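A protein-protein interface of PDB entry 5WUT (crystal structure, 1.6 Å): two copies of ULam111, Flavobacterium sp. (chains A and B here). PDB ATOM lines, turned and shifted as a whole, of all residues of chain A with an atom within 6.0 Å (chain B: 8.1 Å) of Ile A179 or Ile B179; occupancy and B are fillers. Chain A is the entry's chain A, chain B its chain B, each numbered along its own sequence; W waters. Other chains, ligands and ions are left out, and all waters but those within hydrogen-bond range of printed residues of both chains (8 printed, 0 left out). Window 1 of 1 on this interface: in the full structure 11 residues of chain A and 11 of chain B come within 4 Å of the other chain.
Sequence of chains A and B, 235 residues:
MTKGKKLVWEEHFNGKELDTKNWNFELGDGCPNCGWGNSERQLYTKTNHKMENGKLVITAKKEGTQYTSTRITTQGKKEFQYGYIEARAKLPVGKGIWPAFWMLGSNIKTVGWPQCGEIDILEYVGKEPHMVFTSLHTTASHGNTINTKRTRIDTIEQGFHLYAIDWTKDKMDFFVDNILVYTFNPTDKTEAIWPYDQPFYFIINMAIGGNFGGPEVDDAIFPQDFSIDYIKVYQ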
ATOM      1  N   THR A 151      14.748   5.037  24.463  1.00  0.00           N
ATOM      2  CA  THR A 151      15.466   6.278  24.206  1.00  0.00           C
ATOM      3  C   THR A 151      14.841   7.423  24.976  1.00  0.00           C
ATOM      4  O   THR A 151      13.650   7.691  24.859  1.00  0.00           O
ATOM      5  CB  THR A 151      15.491   6.615  22.700  1.00  0.00           C
ATOM      6  OG1 THR A 151      16.106   5.538  21.986  1.00  0.00           O
ATOM      7  CG2 THR A 151      16.281   7.893  22.439  1.00  0.00           C
ATOM      8  N   ARG A 152      15.656   8.090  25.775  1.00  0.00           N
ATOM      9  CA  ARG A 152      15.198   9.246  26.522  1.00  0.00           C
ATOM     10  C   ARG A 152      15.180  10.511  25.681  1.00  0.00           C
ATOM     11  O   ARG A 152      16.179  10.878  25.065  1.00  0.00           O
ATOM     12  CB  ARG A 152      16.071   9.473  27.750  1.00  0.00           C
ATOM     13  CG  ARG A 152      15.720  10.753  28.459  1.00  0.00           C
ATOM     14  CD  ARG A 152      16.541  10.958  29.721  1.00  0.00           C
ATOM     15  NE  ARG A 152      16.449  12.342  30.175  1.00  0.00           N
ATOM     16  CZ  ARG A 152      17.214  12.860  31.132  1.00  0.00           C
ATOM     17  NH1 ARG A 152      18.117  12.102  31.738  1.00  0.00           N
ATOM     18  NH2 ARG A 152      17.076  14.134  31.478  1.00  0.00           N
ATOM     19  N   ILE A 153      14.038  11.190  25.680  1.00  0.00           N
ATOM     20  CA  ILE A 153      13.853  12.426  24.933  1.00  0.00           C
ATOM     21  C   ILE A 153      12.911  13.307  25.741  1.00  0.00           C
ATOM     22  O   ILE A 153      11.695  13.103  25.716  1.00  0.00           O
ATOM     23  CB  ILE A 153      13.259  12.175  23.506  1.00  0.00           C
ATOM     24  CG1 ILE A 153      14.047  11.088  22.765  1.00  0.00           C
ATOM     25  CG2 ILE A 153      13.179  13.472  22.723  1.00  0.00           C
ATOM     26  CD1 ILE A 153      13.549  10.755  21.354  1.00  0.00           C
ATOM     27  N   PHE A 174      16.749   2.595  13.259  1.00  0.00           N
ATOM     28  CA  PHE A 174      15.627   3.381  13.758  1.00  0.00           C
ATOM     29  C   PHE A 174      16.074   4.805  14.076  1.00  0.00           C
ATOM     30  O   PHE A 174      17.129   4.987  14.699  1.00  0.00           O
ATOM     31  CB  PHE A 174      15.038   2.748  15.029  1.00  0.00           C
ATOM     32  CG  PHE A 174      14.424   1.377  14.828  1.00  0.00           C
ATOM     33  CD1 PHE A 174      15.226   0.251  14.670  1.00  0.00           C
ATOM     34  CD2 PHE A 174      13.037   1.208  14.873  1.00  0.00           C
ATOM     35  CE1 PHE A 174      14.649  -1.024  14.513  1.00  0.00           C
ATOM     36  CE2 PHE A 174      12.464  -0.046  14.723  1.00  0.00           C
ATOM     37  CZ  PHE A 174      13.267  -1.161  14.538  1.00  0.00           C
ATOM     38  N   PHE A 175      15.285   5.796  13.660  1.00  0.00           N
ATOM     39  CA  PHE A 175      15.621   7.208  13.845  1.00  0.00           C
ATOM     40  C   PHE A 175      14.510   7.980  14.523  1.00  0.00           C
ATOM     41  O   PHE A 175      13.335   7.815  14.198  1.00  0.00           O
ATOM     42  CB  PHE A 175      15.925   7.894  12.500  1.00  0.00           C
ATOM     43  CG  PHE A 175      16.965   7.206  11.669  1.00  0.00           C
ATOM     44  CD1 PHE A 175      16.638   6.103  10.889  1.00  0.00           C
ATOM     45  CD2 PHE A 175      18.263   7.695  11.612  1.00  0.00           C
ATOM     46  CE1 PHE A 175      17.594   5.476  10.123  1.00  0.00           C
ATOM     47  CE2 PHE A 175      19.220   7.090  10.833  1.00  0.00           C
ATOM     48  CZ  PHE A 175      18.892   5.967  10.081  1.00  0.00           C
ATOM     49  N   VAL A 176      14.877   8.839  15.464  1.00  0.00           N
ATOM     50  CA  VAL A 176      13.938   9.806  15.981  1.00  0.00           C
ATOM     51  C   VAL A 176      14.519  11.182  15.749  1.00  0.00           C
ATOM     52  O   VAL A 176      15.681  11.422  16.086  1.00  0.00           O
ATOM     53  CB  VAL A 176      13.642   9.571  17.478  1.00  0.00           C
ATOM     54  CG1 VAL A 176      12.621  10.587  17.982  1.00  0.00           C
ATOM     55  CG2 VAL A 176      13.116   8.158  17.678  1.00  0.00           C
ATOM     56  N   ASP A 177      13.732  12.061  15.131  1.00  0.00           N
ATOM     57  CA  ASP A 177      14.194  13.390  14.739  1.00  0.00           C
ATOM     58  C   ASP A 177      15.538  13.311  14.032  1.00  0.00           C
ATOM     59  O   ASP A 177      16.435  14.116  14.277  1.00  0.00           O
ATOM     60  CB  ASP A 177      14.264  14.314  15.962  1.00  0.00           C
ATOM     61  CG  ASP A 177      12.895  14.590  16.562  1.00  0.00           C
ATOM     62  OD1 ASP A 177      11.889  14.555  15.831  1.00  0.00           O
ATOM     63  OD2 ASP A 177      12.821  14.850  17.767  1.00  0.00           O
ATOM     64  N   ASN A 178      15.642  12.316  13.152  1.00  0.00           N
ATOM     65  CA  ASN A 178      16.796  12.109  12.272  1.00  0.00           C
ATOM     66  C   ASN A 178      18.042  11.645  13.012  1.00  0.00           C
ATOM     67  O   ASN A 178      19.122  11.609  12.422  1.00  0.00           O
ATOM     68  CB  ASN A 178      17.105  13.389  11.488  1.00  0.00           C
ATOM     69  CG  ASN A 178      15.952  13.825  10.607  1.00  0.00           C
ATOM     70  OD1 ASN A 178      15.469  13.054   9.791  1.00  0.00           O
ATOM     71  ND2 ASN A 178      15.504  15.065  10.775  1.00  0.00           N
ATOM     72  N   ILE A 179      17.899  11.295  14.293  1.00  0.00           N
ATOM     73  CA  ILE A 179      19.016  10.719  15.049  1.00  0.00           C
ATOM     74  C   ILE A 179      18.916   9.191  15.122  1.00  0.00           C
ATOM     75  O   ILE A 179      17.898   8.651  15.538  1.00  0.00           O
ATOM     76  CB  ILE A 179      19.077  11.325  16.447  1.00  0.00           C
ATOM     77  CG1 ILE A 179      19.365  12.817  16.300  1.00  0.00           C
ATOM     78  CG2 ILE A 179      20.126  10.620  17.287  1.00  0.00           C
ATOM     79  CD1 ILE A 179      19.402  13.559  17.591  1.00  0.00           C
ATOM     80  N   LEU A 180      19.962   8.493  14.685  1.00  0.00           N
ATOM     81  CA  LEU A 180      19.956   7.030  14.755  1.00  0.00           C
ATOM     82  C   LEU A 180      19.996   6.583  16.208  1.00  0.00           C
ATOM     83  O   LEU A 180      20.978   6.854  16.914  1.00  0.00           O
ATOM     84  CB  LEU A 180      21.133   6.443  13.993  1.00  0.00           C
ATOM     85  CG  LEU A 180      21.275   4.921  14.039  1.00  0.00           C
ATOM     86  CD1 LEU A 180      20.094   4.277  13.377  1.00  0.00           C
ATOM     87  CD2 LEU A 180      22.576   4.518  13.335  1.00  0.00           C
ATOM     88  N   VAL A 181      18.926   5.931  16.665  1.00  0.00           N
ATOM     89  CA  VAL A 181      18.832   5.560  18.082  1.00  0.00           C
ATOM     90  C   VAL A 181      19.006   4.067  18.346  1.00  0.00           C
ATOM     91  O   VAL A 181      19.284   3.674  19.484  1.00  0.00           O
ATOM     92  CB  VAL A 181      17.497   6.006  18.701  1.00  0.00           C
ATOM     93  CG1 VAL A 181      17.385   7.514  18.645  1.00  0.00           C
ATOM     94  CG2 VAL A 181      16.303   5.332  17.999  1.00  0.00           C
ATOM     95  N   TYR A 182      18.847   3.240  17.314  1.00  0.00           N
ATOM     96  CA  TYR A 182      18.869   1.789  17.495  1.00  0.00           C
ATOM     97  C   TYR A 182      19.104   1.097  16.157  1.00  0.00           C
ATOM     98  O   TYR A 182      18.545   1.505  15.133  1.00  0.00           O
ATOM     99  CB  TYR A 182      17.552   1.296  18.128  1.00  0.00           C
ATOM    100  CG  TYR A 182      17.417  -0.208  18.256  1.00  0.00           C
ATOM    101  CD1 TYR A 182      18.398  -0.974  18.889  1.00  0.00           C
ATOM    102  CD2 TYR A 182      16.287  -0.858  17.777  1.00  0.00           C
ATOM    103  CE1 TYR A 182      18.273  -2.356  18.994  1.00  0.00           C
ATOM    104  CE2 TYR A 182      16.147  -2.235  17.896  1.00  0.00           C
ATOM    105  CZ  TYR A 182      17.137  -2.972  18.504  1.00  0.00           C
ATOM    106  OH  TYR A 182      16.993  -4.343  18.587  1.00  0.00           O
ATOM    107  N   TYR B  84      23.512  20.717  33.875  1.00  0.00           N
ATOM    108  CA  TYR B  84      23.047  20.485  32.517  1.00  0.00           C
ATOM    109  C   TYR B  84      23.608  21.604  31.677  1.00  0.00           C
ATOM    110  O   TYR B  84      23.314  22.775  31.905  1.00  0.00           O
ATOM    111  CB  TYR B  84      21.515  20.435  32.426  1.00  0.00           C
ATOM    112  CG  TYR B  84      21.049  19.885  31.091  1.00  0.00           C
ATOM    113  CD1 TYR B  84      20.866  20.722  30.002  1.00  0.00           C
ATOM    114  CD2 TYR B  84      20.781  18.533  30.930  1.00  0.00           C
ATOM    115  CE1 TYR B  84      20.458  20.224  28.772  1.00  0.00           C
ATOM    116  CE2 TYR B  84      20.360  18.021  29.714  1.00  0.00           C
ATOM    117  CZ  TYR B  84      20.205  18.863  28.636  1.00  0.00           C
ATOM    118  OH  TYR B  84      19.788  18.326  27.424  1.00  0.00           O
ATOM    119  N   VAL B 132      28.372  12.696  14.408  1.00  0.00           N
ATOM    120  CA  VAL B 132      28.989  13.434  15.514  1.00  0.00           C
ATOM    121  C   VAL B 132      29.528  12.449  16.543  1.00  0.00           C
ATOM    122  O   VAL B 132      29.167  11.271  16.530  1.00  0.00           O
ATOM    123  CB  VAL B 132      28.021  14.413  16.194  1.00  0.00           C
ATOM    124  CG1 VAL B 132      27.484  15.428  15.175  1.00  0.00           C
ATOM    125  CG2 VAL B 132      26.897  13.665  16.870  1.00  0.00           C
ATOM    126  N   THR B 151      27.439   8.971  16.659  1.00  0.00           N
ATOM    127  CA  THR B 151      26.010   9.080  16.408  1.00  0.00           C
ATOM    128  C   THR B 151      25.754   9.579  14.990  1.00  0.00           C
ATOM    129  O   THR B 151      26.276  10.618  14.587  1.00  0.00           O
ATOM    130  CB  THR B 151      25.329  10.011  17.418  1.00  0.00           C
ATOM    131  OG1 THR B 151      25.532   9.500  18.744  1.00  0.00           O
ATOM    132  CG2 THR B 151      23.821  10.069  17.167  1.00  0.00           C
ATOM    133  N   ARG B 152      24.974   8.814  14.233  1.00  0.00           N
ATOM    134  CA  ARG B 152      24.580   9.204  12.891  1.00  0.00           C
ATOM    135  C   ARG B 152      23.400  10.159  12.907  1.00  0.00           C
ATOM    136  O   ARG B 152      22.384   9.896  13.537  1.00  0.00           O
ATOM    137  CB  ARG B 152      24.237   7.982  12.039  1.00  0.00           C
ATOM    138  CG  ARG B 152      23.695   8.372  10.685  1.00  0.00           C
ATOM    139  CD  ARG B 152      23.423   7.174   9.813  1.00  0.00           C
ATOM    140  NE  ARG B 152      22.579   7.554   8.686  1.00  0.00           N
ATOM    141  CZ  ARG B 152      22.005   6.678   7.875  1.00  0.00           C
ATOM    142  NH1 ARG B 152      22.199   5.383   8.075  1.00  0.00           N
ATOM    143  NH2 ARG B 152      21.244   7.095   6.871  1.00  0.00           N
ATOM    144  N   ILE B 153      23.559  11.279  12.204  1.00  0.00           N
ATOM    145  CA  ILE B 153      22.532  12.306  12.100  1.00  0.00           C
ATOM    146  C   ILE B 153      22.658  12.943  10.726  1.00  0.00           C
ATOM    147  O   ILE B 153      23.552  13.766  10.507  1.00  0.00           O
ATOM    148  CB  ILE B 153      22.680  13.400  13.185  1.00  0.00           C
ATOM    149  CG1 ILE B 153      22.780  12.789  14.584  1.00  0.00           C
ATOM    150  CG2 ILE B 153      21.515  14.375  13.081  1.00  0.00           C
ATOM    151  CD1 ILE B 153      22.933  13.795  15.693  1.00  0.00           C
ATOM    152  N   ASP B 154      21.811  12.545   9.780  1.00  0.00           N
ATOM    153  CA  ASP B 154      22.013  12.964   8.393  1.00  0.00           C
ATOM    154  C   ASP B 154      21.744  14.444   8.166  1.00  0.00           C
ATOM    155  O   ASP B 154      22.147  15.000   7.146  1.00  0.00           O
ATOM    156  CB  ASP B 154      21.136  12.131   7.455  1.00  0.00           C
ATOM    157  CG  ASP B 154      21.648  10.711   7.284  1.00  0.00           C
ATOM    158  OD1 ASP B 154      22.697  10.358   7.868  1.00  0.00           O
ATOM    159  OD2 ASP B 154      21.005   9.938   6.545  1.00  0.00           O
ATOM    160  N   THR B 155      21.056  15.073   9.112  1.00  0.00           N
ATOM    161  CA  THR B 155      20.698  16.480   9.025  1.00  0.00           C
ATOM    162  C   THR B 155      21.626  17.416   9.801  1.00  0.00           C
ATOM    163  O   THR B 155      21.327  18.607   9.943  1.00  0.00           O
ATOM    164  CB  THR B 155      19.298  16.701   9.575  1.00  0.00           C
ATOM    165  OG1 THR B 155      19.251  16.154  10.899  1.00  0.00           O
ATOM    166  CG2 THR B 155      18.263  16.001   8.696  1.00  0.00           C
ATOM    167  N   ILE B 156      22.730  16.895  10.332  1.00  0.00           N
ATOM    168  CA  ILE B 156      23.495  17.672  11.312  1.00  0.00           C
ATOM    169  C   ILE B 156      24.138  18.920  10.680  1.00  0.00           C
ATOM    170  O   ILE B 156      24.317  19.920  11.367  1.00  0.00           O
ATOM    171  CB  ILE B 156      24.577  16.791  12.046  1.00  0.00           C
ATOM    172  CG1 ILE B 156      25.006  17.433  13.375  1.00  0.00           C
ATOM    173  CG2 ILE B 156      25.794  16.502  11.165  1.00  0.00           C
ATOM    174  CD1 ILE B 156      23.947  17.373  14.454  1.00  0.00           C
ATOM    175  N   HIS B 161      21.866  23.036  15.760  1.00  0.00           N
ATOM    176  CA  HIS B 161      21.486  21.901  16.600  1.00  0.00           C
ATOM    177  C   HIS B 161      21.933  22.129  18.038  1.00  0.00           C
ATOM    178  O   HIS B 161      22.752  23.009  18.306  1.00  0.00           O
ATOM    179  CB  HIS B 161      22.081  20.608  16.034  1.00  0.00           C
ATOM    180  CG  HIS B 161      21.546  20.243  14.684  1.00  0.00           C
ATOM    181  ND1 HIS B 161      20.558  19.296  14.504  1.00  0.00           N
ATOM    182  CD2 HIS B 161      21.843  20.711  13.447  1.00  0.00           C
ATOM    183  CE1 HIS B 161      20.278  19.193  13.219  1.00  0.00           C
ATOM    184  NE2 HIS B 161      21.041  20.045  12.552  1.00  0.00           N
ATOM    185  N   LEU B 162      21.387  21.331  18.954  1.00  0.00           N
ATOM    186  CA  LEU B 162      21.711  21.408  20.373  1.00  0.00           C
ATOM    187  C   LEU B 162      22.636  20.269  20.759  1.00  0.00           C
ATOM    188  O   LEU B 162      22.400  19.116  20.389  1.00  0.00           O
ATOM    189  CB  LEU B 162      20.436  21.348  21.228  1.00  0.00           C
ATOM    190  CG  LEU B 162      19.383  22.402  20.904  1.00  0.00           C
ATOM    191  CD1 LEU B 162      18.142  22.191  21.773  1.00  0.00           C
ATOM    192  CD2 LEU B 162      19.945  23.795  21.107  1.00  0.00           C
ATOM    193  N   ALA B 164      24.534  18.788  24.272  1.00  0.00           N
ATOM    194  CA  ALA B 164      24.429  18.967  25.720  1.00  0.00           C
ATOM    195  C   ALA B 164      24.937  17.785  26.535  1.00  0.00           C
ATOM    196  O   ALA B 164      25.057  16.675  26.031  1.00  0.00           O
ATOM    197  CB  ALA B 164      22.975  19.265  26.095  1.00  0.00           C
ATOM    198  N   ASP B 173      25.700  12.044  30.979  1.00  0.00           N
ATOM    199  CA  ASP B 173      24.762  11.813  29.866  1.00  0.00           C
ATOM    200  C   ASP B 173      25.030  12.812  28.750  1.00  0.00           C
ATOM    201  O   ASP B 173      25.261  13.983  29.026  1.00  0.00           O
ATOM    202  CB  ASP B 173      23.299  11.972  30.312  1.00  0.00           C
ATOM    203  CG  ASP B 173      22.779  10.808  31.158  1.00  0.00           C
ATOM    204  OD1 ASP B 173      21.866  11.056  31.967  1.00  0.00           O
ATOM    205  OD2 ASP B 173      23.219   9.659  30.998  1.00  0.00           O
ATOM    206  N   PHE B 174      24.989  12.366  27.495  1.00  0.00           N
ATOM    207  CA  PHE B 174      25.179  13.257  26.358  1.00  0.00           C
ATOM    208  C   PHE B 174      23.915  13.316  25.495  1.00  0.00           C
ATOM    209  O   PHE B 174      23.327  12.268  25.208  1.00  0.00           O
ATOM    210  CB  PHE B 174      26.359  12.795  25.490  1.00  0.00           C
ATOM    211  CG  PHE B 174      27.704  12.859  26.178  1.00  0.00           C
ATOM    212  CD1 PHE B 174      28.066  11.909  27.124  1.00  0.00           C
ATOM    213  CD2 PHE B 174      28.634  13.826  25.820  1.00  0.00           C
ATOM    214  CE1 PHE B 174      29.322  11.943  27.729  1.00  0.00           C
ATOM    215  CE2 PHE B 174      29.886  13.870  26.426  1.00  0.00           C
ATOM    216  CZ  PHE B 174      30.229  12.938  27.378  1.00  0.00           C
ATOM    217  N   PHE B 175      23.515  14.518  25.073  1.00  0.00           N
ATOM    218  CA  PHE B 175      22.298  14.732  24.279  1.00  0.00           C
ATOM    219  C   PHE B 175      22.585  15.516  23.010  1.00  0.00           C
ATOM    220  O   PHE B 175      23.306  16.511  23.033  1.00  0.00           O
ATOM    221  CB  PHE B 175      21.234  15.504  25.081  1.00  0.00           C
ATOM    222  CG  PHE B 175      20.894  14.904  26.422  1.00  0.00           C
ATOM    223  CD1 PHE B 175      21.703  15.130  27.526  1.00  0.00           C
ATOM    224  CD2 PHE B 175      19.732  14.164  26.595  1.00  0.00           C
ATOM    225  CE1 PHE B 175      21.383  14.588  28.766  1.00  0.00           C
ATOM    226  CE2 PHE B 175      19.396  13.626  27.845  1.00  0.00           C
ATOM    227  CZ  PHE B 175      20.230  13.843  28.926  1.00  0.00           C
ATOM    228  N   VAL B 176      21.991  15.094  21.901  1.00  0.00           N
ATOM    229  CA  VAL B 176      21.987  15.909  20.695  1.00  0.00           C
ATOM    230  C   VAL B 176      20.530  16.151  20.329  1.00  0.00           C
ATOM    231  O   VAL B 176      19.743  15.199  20.277  1.00  0.00           O
ATOM    232  CB  VAL B 176      22.729  15.238  19.521  1.00  0.00           C
ATOM    233  CG1 VAL B 176      22.712  16.129  18.318  1.00  0.00           C
ATOM    234  CG2 VAL B 176      24.168  14.937  19.917  1.00  0.00           C
ATOM    235  N   ASP B 177      20.167  17.417  20.120  1.00  0.00           N
ATOM    236  CA  ASP B 177      18.774  17.816  19.883  1.00  0.00           C
ATOM    237  C   ASP B 177      17.802  17.165  20.880  1.00  0.00           C
ATOM    238  O   ASP B 177      16.710  16.733  20.519  1.00  0.00           O
ATOM    239  CB  ASP B 177      18.356  17.482  18.449  1.00  0.00           C
ATOM    240  CG  ASP B 177      19.139  18.269  17.424  1.00  0.00           C
ATOM    241  OD1 ASP B 177      19.603  19.379  17.764  1.00  0.00           O
ATOM    242  OD2 ASP B 177      19.275  17.794  16.281  1.00  0.00           O
ATOM    243  N   ASN B 178      18.221  17.143  22.148  1.00  0.00           N
ATOM    244  CA  ASN B 178      17.434  16.639  23.278  1.00  0.00           C
ATOM    245  C   ASN B 178      17.259  15.117  23.309  1.00  0.00           C
ATOM    246  O   ASN B 178      16.537  14.588  24.153  1.00  0.00           O
ATOM    247  CB  ASN B 178      16.065  17.319  23.308  1.00  0.00           C
ATOM    248  CG  ASN B 178      16.177  18.811  23.452  1.00  0.00           C
ATOM    249  OD1 ASN B 178      16.834  19.290  24.365  1.00  0.00           O
ATOM    250  ND2 ASN B 178      15.545  19.554  22.548  1.00  0.00           N
ATOM    251  N   ILE B 179      17.953  14.409  22.432  1.00  0.00           N
ATOM    252  CA  ILE B 179      17.948  12.951  22.455  1.00  0.00           C
ATOM    253  C   ILE B 179      19.178  12.402  23.168  1.00  0.00           C
ATOM    254  O   ILE B 179      20.291  12.757  22.814  1.00  0.00           O
ATOM    255  CB  ILE B 179      17.887  12.389  21.033  1.00  0.00           C
ATOM    256  CG1 ILE B 179      16.553  12.821  20.415  1.00  0.00           C
ATOM    257  CG2 ILE B 179      18.064  10.878  21.042  1.00  0.00           C
ATOM    258  CD1 ILE B 179      16.338  12.395  19.001  1.00  0.00           C
ATOM    259  N   LEU B 180      18.978  11.577  24.193  1.00  0.00           N
ATOM    260  CA  LEU B 180      20.097  10.955  24.900  1.00  0.00           C
ATOM    261  C   LEU B 180      20.820   9.960  23.998  1.00  0.00           C
ATOM    262  O   LEU B 180      20.253   8.927  23.636  1.00  0.00           O
ATOM    263  CB  LEU B 180      19.615  10.260  26.171  1.00  0.00           C
ATOM    264  CG  LEU B 180      20.676   9.497  26.972  1.00  0.00           C
ATOM    265  CD1 LEU B 180      21.725  10.442  27.446  1.00  0.00           C
ATOM    266  CD2 LEU B 180      20.010   8.812  28.172  1.00  0.00           C
ATOM    267  N   VAL B 181      22.073  10.265  23.662  1.00  0.00           N
ATOM    268  CA  VAL B 181      22.826   9.434  22.712  1.00  0.00           C
ATOM    269  C   VAL B 181      23.942   8.604  23.333  1.00  0.00           C
ATOM    270  O   VAL B 181      24.427   7.669  22.705  1.00  0.00           O
ATOM    271  CB  VAL B 181      23.447  10.287  21.589  1.00  0.00           C
ATOM    272  CG1 VAL B 181      22.362  10.949  20.759  1.00  0.00           C
ATOM    273  CG2 VAL B 181      24.446  11.331  22.151  1.00  0.00           C
ATOM    274  N   TYR B 182      24.374   8.941  24.545  1.00  0.00           N
ATOM    275  CA  TYR B 182      25.508   8.244  25.166  1.00  0.00           C
ATOM    276  C   TYR B 182      25.528   8.495  26.671  1.00  0.00           C
ATOM    277  O   TYR B 182      25.249   9.602  27.118  1.00  0.00           O
ATOM    278  CB  TYR B 182      26.842   8.686  24.515  1.00  0.00           C
ATOM    279  CG  TYR B 182      28.091   8.122  25.169  1.00  0.00           C
ATOM    280  CD1 TYR B 182      28.258   6.750  25.360  1.00  0.00           C
ATOM    281  CD2 TYR B 182      29.113   8.967  25.582  1.00  0.00           C
ATOM    282  CE1 TYR B 182      29.398   6.247  25.972  1.00  0.00           C
ATOM    283  CE2 TYR B 182      30.264   8.474  26.184  1.00  0.00           C
ATOM    284  CZ  TYR B 182      30.399   7.123  26.383  1.00  0.00           C
ATOM    285  OH  TYR B 182      31.542   6.652  26.987  1.00  0.00           O
HETATM  286  O   HOH W   1      17.265  16.725  15.033  1.00  0.00           O
HETATM  287  O   HOH W   2      14.612  16.611  18.855  1.00  0.00           O
HETATM  288  O   HOH W   3      20.048  10.408  10.234  1.00  0.00           O
HETATM  289  O   HOH W   4      23.719   6.700  16.134  1.00  0.00           O
HETATM  290  O   HOH W   5      18.884   9.509  31.748  1.00  0.00           O
HETATM  291  O   HOH W   6      18.540   7.145  25.154  1.00  0.00           O
HETATM  292  O   HOH W   7      17.268  17.196  12.333  1.00  0.00           O
HETATM  293  O   HOH W   8      20.298  12.970  33.016  1.00  0.00           O
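Of the 12 printed residues of chain A, 8 touch a printed residue of chain B.
Hydrophobic or aromatic side chains of chain A within 4 Å of the printed part of chain B: Ile A153, Phe A175, Ile A179 and Leu A180.
Of the 21 printed residues of chain B, 11 touch a printed residue of chain A.
Hydrophobic or aromatic side chains of chain B that line the printed part of chain A: Ile B153, Phe B175, Ile B179 and Leu B180.
Along chain B the printed residues that touch a printed residue of chain A span positions 151 to 180.
Among the printed residues, 20 pairs touch across the chains.
Among the printed residues, Asp or Glu carboxylates within 4 Å of a Lys or Arg side-chain nitrogen of the other chain: Arg A152 with Asp B173.
Water W1 bridges the side-chain carboxylate (OD2) of Asp B177 and the backbone carbonyl oxygen (O) of Asp A177.
Water W7 lies within hydrogen-bond range of the side-chain hydroxyl (OG1) of Thr B155 (2.7 Å) and the side-chain amide nitrogen (ND2) of Asn A178 (3.2 Å).
Water W3 bridges O of Asn A178 (2.7 Å) and N of Asp B154 (2.8 Å).
Water W2 lies within hydrogen-bond range of the backbone carbonyl oxygen (O) of Asp B177 and the side-chain carboxylate (OD2) of Asp A177.
Water W5 bridges NH1 of Arg A152 (2.7 Å) and OD1 of Asp B173 (3.4 Å).
Water W4 lies within hydrogen-bond range of the backbone carbonyl oxygen (O) of Leu A180 and the backbone NH (N) of Arg B152.
Ile A179 touches just these residues of chain B: Thr B151, Arg B152, Ile B153, Val B176 and Ile B179.
Ile B179 touches five residues of chain A.
Printed residues of chain B within 4 Å of Ile A153: Asn B178 (3.5 Å) and Ile B179 (3.8 Å).
Printed residues of chain B within 4 Å of Asn A178: Arg B152, Ile B153, Asp B154 and Thr B155.
Of the printed residues of chain B, Leu A180 touches Arg B152 (3.0 Å).
Printed residues of chain B within 4 Å of Val A176: Ile B179 (3.1 Å).
Of the printed residues of chain A, Val B176 touches Ile A179.
Phe B174 touches none of the printed residues of chain A.
The nearest residue of chain A that does not touch Ile B179 is Asp A177 (4.1 Å).
The nearest printed residue of chain A that does not touch Asn B178 is Ile A179 (5.9 Å).
The guanidinium group of Arg A152 is in salt-bridge range of the side-chain carboxylate of Asp B173, at 3.9 Å.
The backbone NH (N) of Leu B180 is in hydrogen-bond range of the backbone carbonyl oxygen (O) of Arg A152, at 3.0 Å.
The backbone carbonyl oxygen of Arg B152 sits at hydrogen-bond distance from the backbone NH of Leu A180 (3.0 Å).
Arg A152 touches Asn B178, and with the chains exchanged Asn A178 touches Arg B152.
Arg A152 touches Leu B180, and with the chains exchanged Leu A180 touches Arg B152.
Ile A153 touches Asn B178, and with the chains exchanged Asn A178 touches Ile B153.
Val A176 touches Ile B179, and with the chains exchanged Ile A179 touches Val B176.
The backbone carbonyl oxygen of Val B132 sits at hydrogen-bond distance from the backbone NH of Thr B151, 2.9 Å away.
OD2 of Asp B154 is in salt-bridge range of NH2 of Arg B152.
The backbone carbonyl oxygen (O) of Thr B155 is in hydrogen-bond range of a ring nitrogen (NE2) of His B161, at 3.0 Å.
The backbone carbonyl oxygen of Ala B164 is in hydrogen-bond range of the backbone NH of Phe B175 (2.8 Å).
Thr A151 touches Ile B179 (CG2 to CG2, 3.7 Å).
Phe B175 touches Arg A152 (CZ to CZ, 3.9 Å).
Ile A153 touches Asn B178 (CA to O, 3.5 Å).
CZ of Arg B152 touches CZ of Phe A175, 3.9 Å away.
Val A176 touches Ile B179 (O to CD1, 3.1 Å).
Arg B152 touches Asn A178 (O to O, 3.8 Å).
OG1 of Thr B155 touches CB of Asn A178, 3.5 Å away.
CG2 of Thr B151 touches CG2 of Ile A179, at 3.7 Å.
Ile B153 touches Ile A179 (CD1 to CG1, 3.7 Å).
Ile A179 touches Ile B179 (CD1 to CD1, 3.6 Å).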
